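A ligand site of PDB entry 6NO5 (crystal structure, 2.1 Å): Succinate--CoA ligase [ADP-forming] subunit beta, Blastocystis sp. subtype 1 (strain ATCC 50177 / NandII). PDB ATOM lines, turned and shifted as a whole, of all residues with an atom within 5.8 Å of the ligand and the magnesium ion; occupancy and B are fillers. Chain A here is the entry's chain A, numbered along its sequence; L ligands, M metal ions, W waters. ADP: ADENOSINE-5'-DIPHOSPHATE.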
ATOM      1  N   GLU A   5     -35.149  17.931  -9.313  1.00  0.00           N
ATOM      2  CA  GLU A   5     -33.974  18.347 -10.056  1.00  0.00           C
ATOM      3  C   GLU A   5     -33.142  17.147 -10.490  1.00  0.00           C
ATOM      4  O   GLU A   5     -32.738  17.035 -11.651  1.00  0.00           O
ATOM      5  CB  GLU A   5     -33.135  19.307  -9.218  1.00  0.00           C
ATOM      6  CG  GLU A   5     -31.862  19.776  -9.904  1.00  0.00           C
ATOM      7  CD  GLU A   5     -30.955  20.580  -8.997  1.00  0.00           C
ATOM      8  OE1 GLU A   5     -31.307  20.774  -7.804  1.00  0.00           O
ATOM      9  OE2 GLU A   5     -29.902  21.038  -9.478  1.00  0.00           O
ATOM     10  N   LYS A   9     -32.276  16.409 -14.384  1.00  0.00           N
ATOM     11  CA  LYS A   9     -30.912  16.502 -14.897  1.00  0.00           C
ATOM     12  C   LYS A   9     -30.445  15.171 -15.490  1.00  0.00           C
ATOM     13  O   LYS A   9     -29.761  15.161 -16.517  1.00  0.00           O
ATOM     14  CB  LYS A   9     -29.961  16.951 -13.784  1.00  0.00           C
ATOM     15  CG  LYS A   9     -30.138  18.415 -13.447  1.00  0.00           C
ATOM     16  CD  LYS A   9     -29.036  18.893 -12.547  1.00  0.00           C
ATOM     17  CE  LYS A   9     -29.044  20.413 -12.441  1.00  0.00           C
ATOM     18  NZ  LYS A   9     -28.109  20.830 -11.375  1.00  0.00           N
ATOM     19  N   GLN A  20     -25.314  19.059 -14.623  1.00  0.00           N
ATOM     20  CA  GLN A  20     -24.632  18.656 -13.402  1.00  0.00           C
ATOM     21  C   GLN A  20     -25.628  17.917 -12.511  1.00  0.00           C
ATOM     22  O   GLN A  20     -26.314  18.520 -11.692  1.00  0.00           O
ATOM     23  CB  GLN A  20     -24.029  19.852 -12.673  1.00  0.00           C
ATOM     24  CG  GLN A  20     -23.110  19.439 -11.529  1.00  0.00           C
ATOM     25  CD  GLN A  20     -22.663  20.598 -10.675  1.00  0.00           C
ATOM     26  OE1 GLN A  20     -23.449  21.495 -10.363  1.00  0.00           O
ATOM     27  NE2 GLN A  20     -21.400  20.587 -10.280  1.00  0.00           N
ATOM     28  N   VAL A  48     -21.487  22.201  -3.378  1.00  0.00           N
ATOM     29  CA  VAL A  48     -22.792  22.835  -3.250  1.00  0.00           C
ATOM     30  C   VAL A  48     -23.804  21.763  -2.871  1.00  0.00           C
ATOM     31  O   VAL A  48     -23.866  20.710  -3.502  1.00  0.00           O
ATOM     32  CB  VAL A  48     -23.220  23.549  -4.543  1.00  0.00           C
ATOM     33  CG1 VAL A  48     -24.648  24.073  -4.405  1.00  0.00           C
ATOM     34  CG2 VAL A  48     -22.261  24.678  -4.856  1.00  0.00           C
ATOM     35  N   LYS A  50     -27.767  20.908  -2.445  1.00  0.00           N
ATOM     36  CA  LYS A  50     -29.030  21.377  -3.023  1.00  0.00           C
ATOM     37  C   LYS A  50     -30.172  20.517  -2.496  1.00  0.00           C
ATOM     38  O   LYS A  50     -30.254  19.323  -2.803  1.00  0.00           O
ATOM     39  CB  LYS A  50     -28.959  21.323  -4.550  1.00  0.00           C
ATOM     40  CG  LYS A  50     -27.668  21.853  -5.139  1.00  0.00           C
ATOM     41  CD  LYS A  50     -27.755  21.975  -6.647  1.00  0.00           C
ATOM     42  CE  LYS A  50     -28.607  23.162  -7.066  1.00  0.00           C
ATOM     43  NZ  LYS A  50     -28.726  23.279  -8.538  1.00  0.00           N
ATOM     44  N   ALA A  55     -40.156  22.885  -5.286  1.00  0.00           N
ATOM     45  CA  ALA A  55     -40.433  24.295  -5.079  1.00  0.00           C
ATOM     46  C   ALA A  55     -39.228  25.073  -5.569  1.00  0.00           C
ATOM     47  O   ALA A  55     -38.090  24.612  -5.455  1.00  0.00           O
ATOM     48  CB  ALA A  55     -40.726  24.603  -3.607  1.00  0.00           C
ATOM     49  N   GLY A  56     -39.479  26.270  -6.098  1.00  0.00           N
ATOM     50  CA  GLY A  56     -38.412  27.128  -6.555  1.00  0.00           C
ATOM     51  C   GLY A  56     -37.945  28.077  -5.468  1.00  0.00           C
ATOM     52  O   GLY A  56     -38.429  28.064  -4.337  1.00  0.00           O
ATOM     53  N   GLY A  57     -36.993  28.924  -5.842  1.00  0.00           N
ATOM     54  CA  GLY A  57     -36.459  29.880  -4.892  1.00  0.00           C
ATOM     55  C   GLY A  57     -35.714  29.255  -3.732  1.00  0.00           C
ATOM     56  O   GLY A  57     -35.648  29.854  -2.648  1.00  0.00           O
ATOM     57  N   ARG A  58     -35.146  28.060  -3.921  1.00  0.00           N
ATOM     58  CA  ARG A  58     -34.501  27.370  -2.812  1.00  0.00           C
ATOM     59  C   ARG A  58     -33.314  28.176  -2.276  1.00  0.00           C
ATOM     60  O   ARG A  58     -33.109  28.265  -1.064  1.00  0.00           O
ATOM     61  CB  ARG A  58     -34.035  25.973  -3.244  1.00  0.00           C
ATOM     62  CG  ARG A  58     -35.146  25.039  -3.688  1.00  0.00           C
ATOM     63  CD  ARG A  58     -34.594  23.762  -4.328  1.00  0.00           C
ATOM     64  NE  ARG A  58     -33.833  24.045  -5.539  1.00  0.00           N
ATOM     65  CZ  ARG A  58     -33.167  23.128  -6.248  1.00  0.00           C
ATOM     66  NH1 ARG A  58     -33.161  21.855  -5.866  1.00  0.00           N
ATOM     67  NH2 ARG A  58     -32.516  23.493  -7.340  1.00  0.00           N
ATOM     68  N   GLY A  59     -32.512  28.751  -3.179  1.00  0.00           N
ATOM     69  CA  GLY A  59     -31.310  29.445  -2.747  1.00  0.00           C
ATOM     70  C   GLY A  59     -31.617  30.556  -1.757  1.00  0.00           C
ATOM     71  O   GLY A  59     -30.840  30.800  -0.833  1.00  0.00           O
ATOM     72  N   LYS A  60     -32.739  31.236  -1.945  1.00  0.00           N
ATOM     73  CA  LYS A  60     -33.119  32.368  -1.118  1.00  0.00           C
ATOM     74  C   LYS A  60     -34.045  31.984   0.029  1.00  0.00           C
ATOM     75  O   LYS A  60     -34.461  32.857   0.795  1.00  0.00           O
ATOM     76  CB  LYS A  60     -33.808  33.419  -1.990  1.00  0.00           C
ATOM     77  CG  LYS A  60     -32.879  34.090  -2.997  1.00  0.00           C
ATOM     78  CD  LYS A  60     -33.568  35.248  -3.726  1.00  0.00           C
ATOM     79  CE  LYS A  60     -32.608  35.970  -4.647  1.00  0.00           C
ATOM     80  NZ  LYS A  60     -32.056  35.073  -5.709  1.00  0.00           N
ATOM     81  N   VAL A  71     -29.769  26.143  -1.217  1.00  0.00           N
ATOM     82  CA  VAL A  71     -28.670  25.773  -2.100  1.00  0.00           C
ATOM     83  C   VAL A  71     -27.430  26.436  -1.506  1.00  0.00           C
ATOM     84  O   VAL A  71     -27.281  27.665  -1.590  1.00  0.00           O
ATOM     85  CB  VAL A  71     -28.897  26.247  -3.552  1.00  0.00           C
ATOM     86  CG1 VAL A  71     -27.681  25.934  -4.409  1.00  0.00           C
ATOM     87  CG2 VAL A  71     -30.147  25.589  -4.127  1.00  0.00           C
ATOM     88  N   CYS A 110     -23.031  18.525  -5.062  1.00  0.00           N
ATOM     89  CA  CYS A 110     -22.438  18.903  -6.342  1.00  0.00           C
ATOM     90  C   CYS A 110     -21.084  19.560  -6.121  1.00  0.00           C
ATOM     91  O   CYS A 110     -20.847  20.199  -5.094  1.00  0.00           O
ATOM     92  CB  CYS A 110     -23.343  19.868  -7.124  1.00  0.00           C
ATOM     93  SG  CYS A 110     -24.995  19.237  -7.463  1.00  0.00           S
ATOM     94  N   GLY A 111     -20.205  19.383  -7.093  1.00  0.00           N
ATOM     95  CA  GLY A 111     -18.972  20.152  -7.112  1.00  0.00           C
ATOM     96  C   GLY A 111     -19.244  21.605  -7.434  1.00  0.00           C
ATOM     97  O   GLY A 111     -20.082  21.931  -8.283  1.00  0.00           O
ATOM     98  N   ALA A 112     -18.543  22.494  -6.742  1.00  0.00           N
ATOM     99  CA  ALA A 112     -18.632  23.922  -7.015  1.00  0.00           C
ATOM    100  C   ALA A 112     -17.832  24.258  -8.276  1.00  0.00           C
ATOM    101  O   ALA A 112     -16.681  23.841  -8.414  1.00  0.00           O
ATOM    102  CB  ALA A 112     -18.105  24.727  -5.824  1.00  0.00           C
ATOM    103  N   VAL A 113     -18.460  25.005  -9.180  1.00  0.00           N
ATOM    104  CA  VAL A 113     -17.846  25.377 -10.448  1.00  0.00           C
ATOM    105  C   VAL A 113     -17.898  26.887 -10.620  1.00  0.00           C
ATOM    106  O   VAL A 113     -18.714  27.578 -10.013  1.00  0.00           O
ATOM    107  CB  VAL A 113     -18.518  24.693 -11.666  1.00  0.00           C
ATOM    108  CG1 VAL A 113     -18.396  23.177 -11.566  1.00  0.00           C
ATOM    109  CG2 VAL A 113     -19.983  25.105 -11.767  1.00  0.00           C
ATOM    110  N   ILE A 115     -19.027  29.919 -12.617  1.00  0.00           N
ATOM    111  CA  ILE A 115     -20.108  30.242 -13.527  1.00  0.00           C
ATOM    112  C   ILE A 115     -19.794  31.576 -14.193  1.00  0.00           C
ATOM    113  O   ILE A 115     -19.663  32.603 -13.509  1.00  0.00           O
ATOM    114  CB  ILE A 115     -21.461  30.299 -12.805  1.00  0.00           C
ATOM    115  CG1 ILE A 115     -21.738  28.979 -12.087  1.00  0.00           C
ATOM    116  CG2 ILE A 115     -22.586  30.630 -13.776  1.00  0.00           C
ATOM    117  CD1 ILE A 115     -22.937  29.033 -11.156  1.00  0.00           C
ATOM    118  N   GLU A 118     -25.204  33.209 -16.899  1.00  0.00           N
ATOM    119  CA  GLU A 118     -26.428  32.490 -16.589  1.00  0.00           C
ATOM    120  C   GLU A 118     -27.515  32.895 -17.575  1.00  0.00           C
ATOM    121  O   GLU A 118     -27.802  34.088 -17.735  1.00  0.00           O
ATOM    122  CB  GLU A 118     -26.871  32.769 -15.150  1.00  0.00           C
ATOM    123  CG  GLU A 118     -25.922  32.206 -14.112  1.00  0.00           C
ATOM    124  CD  GLU A 118     -26.481  32.248 -12.709  1.00  0.00           C
ATOM    125  OE1 GLU A 118     -27.613  32.746 -12.525  1.00  0.00           O
ATOM    126  OE2 GLU A 118     -25.792  31.771 -11.775  1.00  0.00           O
ATOM    127  N   ASN A 210     -33.047  27.042 -15.543  1.00  0.00           N
ATOM    128  CA  ASN A 210     -32.830  28.345 -14.910  1.00  0.00           C
ATOM    129  C   ASN A 210     -31.890  28.156 -13.729  1.00  0.00           C
ATOM    130  O   ASN A 210     -32.322  27.881 -12.603  1.00  0.00           O
ATOM    131  CB  ASN A 210     -34.151  28.965 -14.452  1.00  0.00           C
ATOM    132  CG  ASN A 210     -33.986  30.382 -13.942  1.00  0.00           C
ATOM    133  OD1 ASN A 210     -33.042  31.078 -14.308  1.00  0.00           O
ATOM    134  ND2 ASN A 210     -34.908  30.807 -13.086  1.00  0.00           N
ATOM    135  N   PRO A 211     -30.569  28.340 -13.941  1.00  0.00           N
ATOM    136  CA  PRO A 211     -29.915  28.791 -15.173  1.00  0.00           C
ATOM    137  C   PRO A 211     -29.311  27.694 -16.059  1.00  0.00           C
ATOM    138  O   PRO A 211     -28.857  26.652 -15.588  1.00  0.00           O
ATOM    139  CB  PRO A 211     -28.787  29.683 -14.638  1.00  0.00           C
ATOM    140  CG  PRO A 211     -28.388  29.020 -13.353  1.00  0.00           C
ATOM    141  CD  PRO A 211     -29.618  28.294 -12.812  1.00  0.00           C
ATOM    142  N   LEU A 227     -27.467  23.930 -14.865  1.00  0.00           N
ATOM    143  CA  LEU A 227     -27.196  23.994 -13.427  1.00  0.00           C
ATOM    144  C   LEU A 227     -28.454  23.888 -12.578  1.00  0.00           C
ATOM    145  O   LEU A 227     -28.354  23.723 -11.356  1.00  0.00           O
ATOM    146  CB  LEU A 227     -26.450  25.296 -13.110  1.00  0.00           C
ATOM    147  CG  LEU A 227     -25.099  25.407 -13.814  1.00  0.00           C
ATOM    148  CD1 LEU A 227     -24.525  26.800 -13.675  1.00  0.00           C
ATOM    149  CD2 LEU A 227     -24.123  24.370 -13.262  1.00  0.00           C
ATOM    150  N   ASP A 228     -29.623  23.977 -13.207  1.00  0.00           N
ATOM    151  CA  ASP A 228     -30.902  23.713 -12.556  1.00  0.00           C
ATOM    152  C   ASP A 228     -31.784  23.128 -13.650  1.00  0.00           C
ATOM    153  O   ASP A 228     -31.511  23.297 -14.846  1.00  0.00           O
ATOM    154  CB  ASP A 228     -31.511  24.978 -11.957  1.00  0.00           C
ATOM    155  CG  ASP A 228     -32.638  24.678 -10.966  1.00  0.00           C
ATOM    156  OD1 ASP A 228     -32.948  23.491 -10.737  1.00  0.00           O
ATOM    157  OD2 ASP A 228     -33.208  25.649 -10.432  1.00  0.00           O
ATOM    158  N   ALA A 229     -32.853  22.450 -13.255  1.00  0.00           N
ATOM    159  CA  ALA A 229     -33.751  21.875 -14.252  1.00  0.00           C
ATOM    160  C   ALA A 229     -35.101  21.633 -13.617  1.00  0.00           C
ATOM    161  O   ALA A 229     -35.193  21.085 -12.511  1.00  0.00           O
ATOM    162  CB  ALA A 229     -33.190  20.581 -14.832  1.00  0.00           C
HETATM  163  PB  ADP L   1     -33.197  27.526  -7.052  1.00  0.00           P
HETATM  164  O1B ADP L   1     -34.358  26.753  -6.494  1.00  0.00           O
HETATM  165  O2B ADP L   1     -32.638  28.562  -6.082  1.00  0.00           O
HETATM  166  O3B ADP L   1     -33.543  28.242  -8.369  1.00  0.00           O
HETATM  167  PA  ADP L   1     -30.739  26.567  -8.369  1.00  0.00           P
HETATM  168  O1A ADP L   1     -30.430  25.220  -8.875  1.00  0.00           O
HETATM  169  O2A ADP L   1     -31.043  27.625  -9.438  1.00  0.00           O
HETATM  170  O3A ADP L   1     -31.979  26.551  -7.359  1.00  0.00           O
HETATM  171  O5' ADP L   1     -29.507  27.125  -7.485  1.00  0.00           O
HETATM  172  C5' ADP L   1     -29.339  28.505  -7.083  1.00  0.00           C
HETATM  173  C4' ADP L   1     -28.102  29.039  -7.742  1.00  0.00           C
HETATM  174  O4' ADP L   1     -26.933  28.318  -7.304  1.00  0.00           O
HETATM  175  C3' ADP L   1     -28.048  28.929  -9.243  1.00  0.00           C
HETATM  176  O3' ADP L   1     -28.856  29.920  -9.873  1.00  0.00           O
HETATM  177  C2' ADP L   1     -26.552  29.124  -9.517  1.00  0.00           C
HETATM  178  O2' ADP L   1     -26.206  30.497  -9.553  1.00  0.00           O
HETATM  179  C1' ADP L   1     -25.910  28.466  -8.279  1.00  0.00           C
HETATM  180  N9  ADP L   1     -25.322  27.151  -8.541  1.00  0.00           N
HETATM  181  C8  ADP L   1     -25.958  26.024  -8.974  1.00  0.00           C
HETATM  182  N7  ADP L   1     -25.170  24.980  -9.109  1.00  0.00           N
HETATM  183  C5  ADP L   1     -23.920  25.462  -8.727  1.00  0.00           C
HETATM  184  C6  ADP L   1     -22.663  24.844  -8.641  1.00  0.00           C
HETATM  185  N6  ADP L   1     -22.443  23.549  -8.870  1.00  0.00           N
HETATM  186  N1  ADP L   1     -21.617  25.620  -8.252  1.00  0.00           N
HETATM  187  C2  ADP L   1     -21.834  26.903  -7.957  1.00  0.00           C
HETATM  188  N3  ADP L   1     -22.987  27.582  -7.985  1.00  0.00           N
HETATM  189  C4  ADP L   1     -23.997  26.803  -8.379  1.00  0.00           C
HETATM  190 MG    MG M   1     -33.013  27.812 -10.503  1.00  0.00          MG
HETATM  191  O   HOH W   1     -34.977  28.122 -11.164  1.00  0.00           O
HETATM  192  O   HOH W   2     -36.244  28.930  -8.638  1.00  0.00           O
HETATM  193  O   HOH W   3     -32.286  29.746 -10.304  1.00  0.00           O
HETATM  194  O   HOH W   4     -25.986  22.249 -10.023  1.00  0.00           O
HETATM  195  O   HOH W   5     -22.553  30.141  -7.306  1.00  0.00           O
HETATM  196  O   HOH W   6     -35.493  25.248  -8.563  1.00  0.00           O
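An oxygen (O2') of the ligand sits at hydrogen-bond distance from the side-chain carboxylate (OE2) of Glu 118, at 2.6 Å. The side-chain amino group (NZ) of Lys 50 lies within salt-bridge range of an oxygen (O1A) of the ligand. N6 of the ligand is in hydrogen-bond range of OE1 of Gln 20 (2.7 Å). An oxygen (O2B) of the ligand sits at hydrogen-bond distance from the backbone NH (N) of Gly 59 (2.9 Å). The backbone NH of Arg 58 sits at hydrogen-bond distance from an oxygen (O1B) of the ligand. An oxygen (O1B) of the ligand lies within salt-bridge range of the guanidinium group of Arg 58 (2.9 Å). The backbone carbonyl oxygen (O) of Gly 111 sits at hydrogen-bond distance from a nitrogen (N6) of the ligand (2.9 Å). N of Val 113 sits at hydrogen-bond distance from N1 of the ligand, 3.3 Å away. N of Gly 57 is in hydrogen-bond range of O1B of the ligand (3.5 Å).
NH2 of Arg 58 lies within salt-bridge range of OD1 of Asp 228 (3.4 Å). The side-chain amino group of Lys 50 lies within hydrogen-bond range of the backbone carbonyl oxygen of Leu 227, 2.9 Å away. The side-chain amino group (NZ) of Lys 50 lies within salt-bridge range of the side-chain carboxylate (OE2) of Glu 5 (2.7 Å). NE2 of Gln 20 lies within hydrogen-bond range of O of Gly 111, 2.7 Å away. O of Gln 20 sits close to NZ of Lys 9. NH1 of Arg 58 lies within salt-bridge range of OE1 of Glu 5 (2.9 Å). O of Leu 227 is in hydrogen-bond range of NZ of Lys 9. N of Val 48 sits at hydrogen-bond distance from O of Cys 110, 2.7 Å away.
Val 48 touches the ligand (CG2 to N1, 3.6 Å). Gly 56 touches the ligand. Val 71 touches the ligand (CG2 to O5', 3.7 Å). Ala 112 touches the ligand. Ile 115 touches the ligand. Pro 211 touches the ligand (CD to O3', 3.4 Å). Leu 227 touches the ligand (O to O1A, 3.6 Å). Hydrophobic or aromatic side chains that line the ligand: Val 48, Val 71, Val 113, Ile 115 and Pro 211. The nearest printed residue that does not touch the ligand is Cys 110 (4.2 Å).
Within 4 Å of the magnesium ion: Asn 210 and Asp 228. The nearest printed residue that does not touch the magnesium ion is Pro 211 (4.1 Å).
Water W3 is bound to the magnesium ion, 2.1 Å away. The magnesium ion is bound by water W1 (2.1 Å). The side-chain carboxylate (OD2) of Asp 228 is bound to the magnesium ion (2.2 Å). O of Asn 210 binds the magnesium ion, at 2.2 Å. O3B of the ligand is bound to the magnesium ion, at 2.2 Å. The magnesium ion is bound by O2A of the ligand, at 2.2 Å.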
